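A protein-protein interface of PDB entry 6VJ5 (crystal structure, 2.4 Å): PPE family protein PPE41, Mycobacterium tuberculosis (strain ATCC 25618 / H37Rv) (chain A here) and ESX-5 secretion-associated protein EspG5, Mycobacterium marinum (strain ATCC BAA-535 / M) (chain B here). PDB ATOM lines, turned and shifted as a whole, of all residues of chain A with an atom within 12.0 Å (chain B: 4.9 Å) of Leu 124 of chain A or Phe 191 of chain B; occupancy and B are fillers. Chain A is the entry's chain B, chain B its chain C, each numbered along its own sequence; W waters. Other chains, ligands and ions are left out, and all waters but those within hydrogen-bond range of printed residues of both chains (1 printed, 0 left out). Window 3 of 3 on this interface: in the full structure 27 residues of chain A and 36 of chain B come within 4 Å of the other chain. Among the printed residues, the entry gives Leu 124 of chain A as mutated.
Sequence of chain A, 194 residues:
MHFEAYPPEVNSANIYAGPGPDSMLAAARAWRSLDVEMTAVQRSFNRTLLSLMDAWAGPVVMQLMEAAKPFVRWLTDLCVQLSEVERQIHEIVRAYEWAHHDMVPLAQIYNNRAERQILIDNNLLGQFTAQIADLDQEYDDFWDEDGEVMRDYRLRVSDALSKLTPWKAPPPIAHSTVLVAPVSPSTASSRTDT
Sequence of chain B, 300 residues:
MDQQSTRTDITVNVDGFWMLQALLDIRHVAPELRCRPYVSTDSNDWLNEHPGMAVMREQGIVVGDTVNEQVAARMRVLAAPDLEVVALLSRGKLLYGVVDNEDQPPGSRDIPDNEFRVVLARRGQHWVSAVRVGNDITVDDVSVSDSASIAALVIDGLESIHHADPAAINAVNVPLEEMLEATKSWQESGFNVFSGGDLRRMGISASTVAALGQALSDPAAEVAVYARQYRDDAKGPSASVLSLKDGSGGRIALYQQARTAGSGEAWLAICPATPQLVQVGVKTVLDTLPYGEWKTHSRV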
ATOM      1  N   ARG A 116      22.881   2.895 -22.939  1.00  0.00           N
ATOM      2  CA  ARG A 116      23.066   2.016 -21.793  1.00  0.00           C
ATOM      3  C   ARG A 116      21.940   0.999 -21.698  1.00  0.00           C
ATOM      4  O   ARG A 116      22.189  -0.181 -21.429  1.00  0.00           O
ATOM      5  CB  ARG A 116      23.154   2.845 -20.516  1.00  0.00           C
ATOM      6  CG  ARG A 116      23.527   2.055 -19.283  1.00  0.00           C
ATOM      7  CD  ARG A 116      23.151   2.823 -18.019  1.00  0.00           C
ATOM      8  NE  ARG A 116      23.920   2.359 -16.873  1.00  0.00           N
ATOM      9  CZ  ARG A 116      23.610   1.287 -16.154  1.00  0.00           C
ATOM     10  NH1 ARG A 116      22.538   0.563 -16.456  1.00  0.00           N
ATOM     11  NH2 ARG A 116      24.376   0.940 -15.128  1.00  0.00           N
ATOM     12  N   GLN A 117      20.698   1.427 -21.930  1.00  0.00           N
ATOM     13  CA  GLN A 117      19.582   0.498 -21.815  1.00  0.00           C
ATOM     14  C   GLN A 117      19.573  -0.512 -22.958  1.00  0.00           C
ATOM     15  O   GLN A 117      19.054  -1.620 -22.796  1.00  0.00           O
ATOM     16  CB  GLN A 117      18.255   1.256 -21.780  1.00  0.00           C
ATOM     17  CG  GLN A 117      17.081   0.426 -21.262  1.00  0.00           C
ATOM     18  CD  GLN A 117      17.268  -0.017 -19.816  1.00  0.00           C
ATOM     19  OE1 GLN A 117      17.381   0.809 -18.908  1.00  0.00           O
ATOM     20  NE2 GLN A 117      17.311  -1.329 -19.601  1.00  0.00           N
ATOM     21  N   ILE A 118      20.123  -0.149 -24.118  1.00  0.00           N
ATOM     22  CA  ILE A 118      20.181  -1.100 -25.223  1.00  0.00           C
ATOM     23  C   ILE A 118      21.194  -2.194 -24.925  1.00  0.00           C
ATOM     24  O   ILE A 118      20.994  -3.358 -25.290  1.00  0.00           O
ATOM     25  CB  ILE A 118      20.502  -0.382 -26.546  1.00  0.00           C
ATOM     26  CG1 ILE A 118      19.314   0.479 -26.962  1.00  0.00           C
ATOM     27  CG2 ILE A 118      20.825  -1.387 -27.636  1.00  0.00           C
ATOM     28  CD1 ILE A 118      19.493   1.187 -28.281  1.00  0.00           C
ATOM     29  N   LEU A 119      22.299  -1.843 -24.267  1.00  0.00           N
ATOM     30  CA  LEU A 119      23.241  -2.870 -23.843  1.00  0.00           C
ATOM     31  C   LEU A 119      22.641  -3.735 -22.742  1.00  0.00           C
ATOM     32  O   LEU A 119      22.826  -4.958 -22.736  1.00  0.00           O
ATOM     33  CB  LEU A 119      24.541  -2.230 -23.370  1.00  0.00           C
ATOM     34  CG  LEU A 119      25.326  -1.409 -24.389  1.00  0.00           C
ATOM     35  CD1 LEU A 119      26.651  -0.955 -23.744  1.00  0.00           C
ATOM     36  CD2 LEU A 119      25.572  -2.150 -25.681  1.00  0.00           C
ATOM     37  N   ILE A 120      21.914  -3.122 -21.803  1.00  0.00           N
ATOM     38  CA  ILE A 120      21.250  -3.897 -20.758  1.00  0.00           C
ATOM     39  C   ILE A 120      20.292  -4.899 -21.386  1.00  0.00           C
ATOM     40  O   ILE A 120      20.328  -6.099 -21.082  1.00  0.00           O
ATOM     41  CB  ILE A 120      20.519  -2.963 -19.777  1.00  0.00           C
ATOM     42  CG1 ILE A 120      21.524  -2.049 -19.078  1.00  0.00           C
ATOM     43  CG2 ILE A 120      19.726  -3.771 -18.758  1.00  0.00           C
ATOM     44  CD1 ILE A 120      22.283  -2.728 -17.975  1.00  0.00           C
ATOM     45  N   ASP A 121      19.436  -4.422 -22.295  1.00  0.00           N
ATOM     46  CA  ASP A 121      18.442  -5.272 -22.934  1.00  0.00           C
ATOM     47  C   ASP A 121      19.060  -6.394 -23.760  1.00  0.00           C
ATOM     48  O   ASP A 121      18.319  -7.257 -24.246  1.00  0.00           O
ATOM     49  CB  ASP A 121      17.531  -4.453 -23.858  1.00  0.00           C
ATOM     50  CG  ASP A 121      16.720  -3.399 -23.121  1.00  0.00           C
ATOM     51  OD1 ASP A 121      16.397  -3.596 -21.927  1.00  0.00           O
ATOM     52  OD2 ASP A 121      16.394  -2.367 -23.752  1.00  0.00           O
ATOM     53  N   ASN A 122      20.386  -6.388 -23.954  1.00  0.00           N
ATOM     54  CA  ASN A 122      21.058  -7.436 -24.713  1.00  0.00           C
ATOM     55  C   ASN A 122      22.206  -8.070 -23.933  1.00  0.00           C
ATOM     56  O   ASN A 122      23.105  -8.653 -24.545  1.00  0.00           O
ATOM     57  CB  ASN A 122      21.596  -6.901 -26.048  1.00  0.00           C
ATOM     58  CG  ASN A 122      20.500  -6.473 -26.993  1.00  0.00           C
ATOM     59  OD1 ASN A 122      19.986  -7.277 -27.768  1.00  0.00           O
ATOM     60  ND2 ASN A 122      20.138  -5.198 -26.940  1.00  0.00           N
ATOM     61  N   ASN A 123      22.199  -7.980 -22.600  1.00  0.00           N
ATOM     62  CA  ASN A 123      23.312  -8.449 -21.786  1.00  0.00           C
ATOM     63  C   ASN A 123      22.995  -9.748 -21.047  1.00  0.00           C
ATOM     64  O   ASN A 123      23.519  -9.982 -19.957  1.00  0.00           O
ATOM     65  CB  ASN A 123      23.725  -7.360 -20.796  1.00  0.00           C
ATOM     66  CG  ASN A 123      25.151  -7.523 -20.320  1.00  0.00           C
ATOM     67  OD1 ASN A 123      26.024  -7.965 -21.080  1.00  0.00           O
ATOM     68  ND2 ASN A 123      25.398  -7.181 -19.057  1.00  0.00           N
ATOM     69  N   LEU A 124      22.173 -10.612 -21.640  1.00  0.00           N
ATOM     70  CA  LEU A 124      21.870 -11.891 -21.007  1.00  0.00           C
ATOM     71  C   LEU A 124      23.134 -12.704 -20.762  1.00  0.00           C
ATOM     72  O   LEU A 124      23.270 -13.350 -19.716  1.00  0.00           O
ATOM     73  CB  LEU A 124      20.900 -12.676 -21.880  1.00  0.00           C
ATOM     74  CG  LEU A 124      19.533 -13.002 -21.279  1.00  0.00           C
ATOM     75  CD1 LEU A 124      18.819 -13.950 -22.244  1.00  0.00           C
ATOM     76  CD2 LEU A 124      19.633 -13.585 -19.896  1.00  0.00           C
ATOM     77  N   LEU A 125      24.060 -12.701 -21.718  1.00  0.00           N
ATOM     78  CA  LEU A 125      25.320 -13.425 -21.588  1.00  0.00           C
ATOM     79  C   LEU A 125      26.436 -12.566 -21.004  1.00  0.00           C
ATOM     80  O   LEU A 125      27.573 -13.037 -20.899  1.00  0.00           O
ATOM     81  CB  LEU A 125      25.746 -13.979 -22.950  1.00  0.00           C
ATOM     82  CG  LEU A 125      24.667 -14.828 -23.626  1.00  0.00           C
ATOM     83  CD1 LEU A 125      25.062 -15.179 -25.049  1.00  0.00           C
ATOM     84  CD2 LEU A 125      24.384 -16.100 -22.830  1.00  0.00           C
ATOM     85  N   GLY A 126      26.142 -11.321 -20.637  1.00  0.00           N
ATOM     86  CA  GLY A 126      27.037 -10.518 -19.833  1.00  0.00           C
ATOM     87  C   GLY A 126      28.209  -9.892 -20.552  1.00  0.00           C
ATOM     88  O   GLY A 126      29.015  -9.218 -19.899  1.00  0.00           O
ATOM     89  N   GLN A 127      28.324 -10.062 -21.865  1.00  0.00           N
ATOM     90  CA  GLN A 127      29.516  -9.626 -22.581  1.00  0.00           C
ATOM     91  C   GLN A 127      29.530  -8.139 -22.906  1.00  0.00           C
ATOM     92  O   GLN A 127      30.490  -7.673 -23.529  1.00  0.00           O
ATOM     93  CB  GLN A 127      29.663 -10.424 -23.875  1.00  0.00           C
ATOM     94  CG  GLN A 127      29.775 -11.903 -23.637  1.00  0.00           C
ATOM     95  CD  GLN A 127      30.883 -12.233 -22.670  1.00  0.00           C
ATOM     96  OE1 GLN A 127      32.059 -11.990 -22.947  1.00  0.00           O
ATOM     97  NE2 GLN A 127      30.510 -12.769 -21.509  1.00  0.00           N
ATOM     98  N   PHE A 128      28.503  -7.389 -22.514  1.00  0.00           N
ATOM     99  CA  PHE A 128      28.507  -5.940 -22.640  1.00  0.00           C
ATOM    100  C   PHE A 128      28.685  -5.244 -21.298  1.00  0.00           C
ATOM    101  O   PHE A 128      28.697  -4.011 -21.248  1.00  0.00           O
ATOM    102  CB  PHE A 128      27.214  -5.465 -23.308  1.00  0.00           C
ATOM    103  CG  PHE A 128      26.981  -6.068 -24.654  1.00  0.00           C
ATOM    104  CD1 PHE A 128      27.766  -5.701 -25.734  1.00  0.00           C
ATOM    105  CD2 PHE A 128      25.975  -6.997 -24.844  1.00  0.00           C
ATOM    106  CE1 PHE A 128      27.555  -6.252 -26.985  1.00  0.00           C
ATOM    107  CE2 PHE A 128      25.756  -7.559 -26.098  1.00  0.00           C
ATOM    108  CZ  PHE A 128      26.550  -7.185 -27.168  1.00  0.00           C
ATOM    109  N   THR A 129      28.849  -6.003 -20.213  1.00  0.00           N
ATOM    110  CA  THR A 129      28.906  -5.403 -18.884  1.00  0.00           C
ATOM    111  C   THR A 129      29.949  -4.294 -18.817  1.00  0.00           C
ATOM    112  O   THR A 129      29.691  -3.214 -18.279  1.00  0.00           O
ATOM    113  CB  THR A 129      29.198  -6.480 -17.839  1.00  0.00           C
ATOM    114  OG1 THR A 129      28.239  -7.536 -17.967  1.00  0.00           O
ATOM    115  CG2 THR A 129      29.127  -5.900 -16.434  1.00  0.00           C
ATOM    116  N   ALA A 130      31.141  -4.539 -19.368  1.00  0.00           N
ATOM    117  CA  ALA A 130      32.199  -3.536 -19.274  1.00  0.00           C
ATOM    118  C   ALA A 130      31.836  -2.273 -20.047  1.00  0.00           C
ATOM    119  O   ALA A 130      32.059  -1.158 -19.561  1.00  0.00           O
ATOM    120  CB  ALA A 130      33.522  -4.113 -19.773  1.00  0.00           C
ATOM    121  N   ILE A 132      28.940  -1.211 -20.467  1.00  0.00           N
ATOM    122  CA  ILE A 132      27.952  -0.516 -19.652  1.00  0.00           C
ATOM    123  C   ILE A 132      28.651   0.374 -18.638  1.00  0.00           C
ATOM    124  O   ILE A 132      28.287   1.541 -18.458  1.00  0.00           O
ATOM    125  CB  ILE A 132      27.012  -1.534 -18.984  1.00  0.00           C
ATOM    126  CG1 ILE A 132      26.111  -2.169 -20.048  1.00  0.00           C
ATOM    127  CG2 ILE A 132      26.201  -0.865 -17.890  1.00  0.00           C
ATOM    128  CD1 ILE A 132      25.421  -3.432 -19.598  1.00  0.00           C
ATOM    129  N   LYS B  93      18.314 -12.315 -10.356  1.00  0.00           N
ATOM    130  CA  LYS B  93      18.806 -11.827 -11.638  1.00  0.00           C
ATOM    131  C   LYS B  93      19.671 -10.586 -11.440  1.00  0.00           C
ATOM    132  O   LYS B  93      19.335  -9.689 -10.662  1.00  0.00           O
ATOM    133  CB  LYS B  93      17.646 -11.517 -12.585  1.00  0.00           C
ATOM    134  CG  LYS B  93      18.110 -11.034 -13.952  1.00  0.00           C
ATOM    135  CD  LYS B  93      16.955 -10.850 -14.922  1.00  0.00           C
ATOM    136  CE  LYS B  93      17.436 -10.206 -16.222  1.00  0.00           C
ATOM    137  NZ  LYS B  93      18.499 -11.001 -16.903  1.00  0.00           N
ATOM    138  N   THR B 183      20.296 -16.681 -28.715  1.00  0.00           N
ATOM    139  CA  THR B 183      19.855 -16.492 -27.339  1.00  0.00           C
ATOM    140  C   THR B 183      18.733 -15.461 -27.258  1.00  0.00           C
ATOM    141  O   THR B 183      17.776 -15.637 -26.496  1.00  0.00           O
ATOM    142  CB  THR B 183      21.034 -16.063 -26.467  1.00  0.00           C
ATOM    143  OG1 THR B 183      22.081 -17.037 -26.546  1.00  0.00           O
ATOM    144  CG2 THR B 183      20.594 -15.919 -25.029  1.00  0.00           C
ATOM    145  N   TRP B 186      15.548 -17.099 -28.403  1.00  0.00           N
ATOM    146  CA  TRP B 186      15.085 -18.080 -27.424  1.00  0.00           C
ATOM    147  C   TRP B 186      14.431 -17.389 -26.238  1.00  0.00           C
ATOM    148  O   TRP B 186      13.375 -17.821 -25.760  1.00  0.00           O
ATOM    149  CB  TRP B 186      16.251 -18.948 -26.957  1.00  0.00           C
ATOM    150  CG  TRP B 186      15.826 -20.192 -26.239  1.00  0.00           C
ATOM    151  CD1 TRP B 186      14.637 -20.847 -26.365  1.00  0.00           C
ATOM    152  CD2 TRP B 186      16.589 -20.930 -25.279  1.00  0.00           C
ATOM    153  NE1 TRP B 186      14.611 -21.946 -25.543  1.00  0.00           N
ATOM    154  CE2 TRP B 186      15.799 -22.019 -24.864  1.00  0.00           C
ATOM    155  CE3 TRP B 186      17.865 -20.775 -24.730  1.00  0.00           C
ATOM    156  CZ2 TRP B 186      16.241 -22.946 -23.927  1.00  0.00           C
ATOM    157  CZ3 TRP B 186      18.304 -21.698 -23.801  1.00  0.00           C
ATOM    158  CH2 TRP B 186      17.495 -22.770 -23.410  1.00  0.00           C
ATOM    159  N   GLN B 187      15.047 -16.313 -25.751  1.00  0.00           N
ATOM    160  CA  GLN B 187      14.425 -15.493 -24.719  1.00  0.00           C
ATOM    161  C   GLN B 187      13.075 -14.964 -25.181  1.00  0.00           C
ATOM    162  O   GLN B 187      12.104 -14.965 -24.416  1.00  0.00           O
ATOM    163  CB  GLN B 187      15.360 -14.339 -24.361  1.00  0.00           C
ATOM    164  CG  GLN B 187      14.860 -13.378 -23.302  1.00  0.00           C
ATOM    165  CD  GLN B 187      15.690 -12.103 -23.273  1.00  0.00           C
ATOM    166  OE1 GLN B 187      15.988 -11.523 -24.319  1.00  0.00           O
ATOM    167  NE2 GLN B 187      16.084 -11.673 -22.076  1.00  0.00           N
ATOM    168  N   SER B 189      10.978 -16.246 -27.198  1.00  0.00           N
ATOM    169  CA  SER B 189       9.992 -17.317 -27.154  1.00  0.00           C
ATOM    170  C   SER B 189       9.617 -17.713 -25.733  1.00  0.00           C
ATOM    171  O   SER B 189       8.814 -18.635 -25.554  1.00  0.00           O
ATOM    172  CB  SER B 189      10.510 -18.553 -27.900  1.00  0.00           C
ATOM    173  OG  SER B 189      11.404 -19.306 -27.096  1.00  0.00           O
ATOM    174  N   GLY B 190      10.168 -17.040 -24.726  1.00  0.00           N
ATOM    175  CA  GLY B 190       9.965 -17.453 -23.352  1.00  0.00           C
ATOM    176  C   GLY B 190      10.854 -18.584 -22.893  1.00  0.00           C
ATOM    177  O   GLY B 190      10.576 -19.185 -21.851  1.00  0.00           O
ATOM    178  N   PHE B 191      11.923 -18.888 -23.633  1.00  0.00           N
ATOM    179  CA  PHE B 191      12.797 -20.021 -23.326  1.00  0.00           C
ATOM    180  C   PHE B 191      12.047 -21.341 -23.487  1.00  0.00           C
ATOM    181  O   PHE B 191      12.215 -22.273 -22.701  1.00  0.00           O
ATOM    182  CB  PHE B 191      13.402 -19.892 -21.927  1.00  0.00           C
ATOM    183  CG  PHE B 191      14.373 -18.754 -21.810  1.00  0.00           C
ATOM    184  CD1 PHE B 191      15.661 -18.870 -22.311  1.00  0.00           C
ATOM    185  CD2 PHE B 191      13.988 -17.555 -21.234  1.00  0.00           C
ATOM    186  CE1 PHE B 191      16.552 -17.815 -22.222  1.00  0.00           C
ATOM    187  CE2 PHE B 191      14.876 -16.495 -21.142  1.00  0.00           C
ATOM    188  CZ  PHE B 191      16.159 -16.627 -21.636  1.00  0.00           C
ATOM    189  N   ASN B 192      11.227 -21.418 -24.531  1.00  0.00           N
ATOM    190  CA  ASN B 192      10.393 -22.587 -24.752  1.00  0.00           C
ATOM    191  C   ASN B 192      11.246 -23.804 -25.080  1.00  0.00           C
ATOM    192  O   ASN B 192      12.156 -23.735 -25.914  1.00  0.00           O
ATOM    193  CB  ASN B 192       9.407 -22.319 -25.882  1.00  0.00           C
ATOM    194  CG  ASN B 192       8.409 -23.438 -26.056  1.00  0.00           C
ATOM    195  OD1 ASN B 192       8.377 -24.100 -27.092  1.00  0.00           O
ATOM    196  ND2 ASN B 192       7.597 -23.672 -25.030  1.00  0.00           N
ATOM    197  N   VAL B 193      10.916 -24.929 -24.444  1.00  0.00           N
ATOM    198  CA  VAL B 193      11.712 -26.140 -24.569  1.00  0.00           C
ATOM    199  C   VAL B 193      11.761 -26.656 -25.996  1.00  0.00           C
ATOM    200  O   VAL B 193      12.649 -27.449 -26.329  1.00  0.00           O
ATOM    201  CB  VAL B 193      11.150 -27.227 -23.629  1.00  0.00           C
ATOM    202  CG1 VAL B 193      11.142 -26.740 -22.190  1.00  0.00           C
ATOM    203  CG2 VAL B 193       9.745 -27.625 -24.076  1.00  0.00           C
ATOM    204  N   GLY B 213      19.096 -22.672 -20.256  1.00  0.00           N
ATOM    205  CA  GLY B 213      17.770 -22.079 -20.188  1.00  0.00           C
ATOM    206  C   GLY B 213      17.341 -21.784 -18.765  1.00  0.00           C
ATOM    207  O   GLY B 213      16.679 -20.779 -18.500  1.00  0.00           O
ATOM    208  N   LEU B 216      19.526 -18.716 -17.445  1.00  0.00           N
ATOM    209  CA  LEU B 216      19.137 -17.456 -18.067  1.00  0.00           C
ATOM    210  C   LEU B 216      17.710 -17.060 -17.716  1.00  0.00           C
ATOM    211  O   LEU B 216      17.396 -15.865 -17.663  1.00  0.00           O
ATOM    212  CB  LEU B 216      19.267 -17.553 -19.589  1.00  0.00           C
ATOM    213  CG  LEU B 216      20.627 -17.929 -20.178  1.00  0.00           C
ATOM    214  CD1 LEU B 216      20.537 -18.002 -21.700  1.00  0.00           C
ATOM    215  CD2 LEU B 216      21.682 -16.928 -19.737  1.00  0.00           C
ATOM    216  N   SER B 217      16.837 -18.040 -17.488  1.00  0.00           N
ATOM    217  CA  SER B 217      15.413 -17.797 -17.300  1.00  0.00           C
ATOM    218  C   SER B 217      15.061 -17.463 -15.857  1.00  0.00           C
ATOM    219  O   SER B 217      14.172 -16.640 -15.615  1.00  0.00           O
ATOM    220  CB  SER B 217      14.626 -19.027 -17.760  1.00  0.00           C
ATOM    221  OG  SER B 217      13.235 -18.861 -17.576  1.00  0.00           O
ATOM    222  N   LYS B 245      26.423 -17.943 -13.551  1.00  0.00           N
ATOM    223  CA  LYS B 245      24.990 -17.940 -13.292  1.00  0.00           C
ATOM    224  C   LYS B 245      24.575 -19.229 -12.601  1.00  0.00           C
ATOM    225  O   LYS B 245      25.050 -20.312 -12.955  1.00  0.00           O
ATOM    226  CB  LYS B 245      24.188 -17.789 -14.590  1.00  0.00           C
ATOM    227  CG  LYS B 245      24.505 -16.534 -15.384  1.00  0.00           C
ATOM    228  CD  LYS B 245      23.762 -16.531 -16.713  1.00  0.00           C
ATOM    229  CE  LYS B 245      24.151 -15.338 -17.568  1.00  0.00           C
ATOM    230  NZ  LYS B 245      23.765 -14.048 -16.933  1.00  0.00           N
HETATM  231  O   HOH W   1      23.244 -11.220 -17.573  1.00  0.00           O
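Printed residues of chain A that touch a printed residue of chain B: Leu 124 and Leu 125.
Among the printed residues, 6 pairs touch across the chains.
Among the printed residues, no Asp or Glu carboxylate lies within 4 Å of a Lys or Arg side-chain nitrogen of the other chain.
Leu 124 of chain A touches just these residues of chain B: Thr 183, Gln 187, Phe 191, Leu 216 and Lys 245.
Phe 191 of chain B touches just one residue of chain A: Leu 124 (3.8 Å).
No residue of chain A comes within 4 Å of Trp 186 of chain B.
No residue of chain A comes within 4 Å of Ser 189 of chain B.
No residue of chain A comes within 4 Å of Gly 190 of chain B.
No residue of chain A comes within 4 Å of Asn 192 of chain B.
No residue of chain A comes within 4 Å of Val 193 of chain B.
No residue of chain A comes within 4 Å of Gly 213 of chain B.
Of chain A, only Leu 124 (3.9 Å) comes within 4 Å of Leu 216 of chain B.
No residue of chain A comes within 4 Å of Ser 217 of chain B.
Of the printed residues of chain B, Leu 125 of chain A touches Thr 183 (3.8 Å).
Of the printed residues of chain A, Lys 245 of chain B touches Leu 124.
The nearest printed residue of chain B that does not touch Leu 125 of chain A is Leu 216 of chain B (4.2 Å).
The side-chain amino group (NZ) of Lys 245 of chain B sits at hydrogen-bond distance from the backbone carbonyl oxygen (O) of Leu 124 of chain A, at 2.9 Å.
Water W1 lies within hydrogen-bond range of O of Asn 123 of chain A (2.7 Å), NZ of Lys 245 of chain B (2.9 Å) and O of Leu 124 of chain A (3.0 Å).
O of Leu 125 of chain A sits at hydrogen-bond distance from NE2 of Gln 127 of chain A (3.0 Å).
The backbone carbonyl oxygen (O) of Trp 186 of chain B lies within hydrogen-bond range of the backbone NH (N) of Phe 191 of chain B, 2.8 Å away.
CD1 of Leu 124 of chain A touches CG2 of Thr 183 of chain B (3.8 Å).
Leu 124 of chain A touches Gln 187 of chain B.
CD1 of Leu 124 of chain A touches CZ of Phe 191 of chain B, 3.8 Å away.
Leu 124 of chain A touches Leu 216 of chain B.
Leu 125 of chain A touches Thr 183 of chain B.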
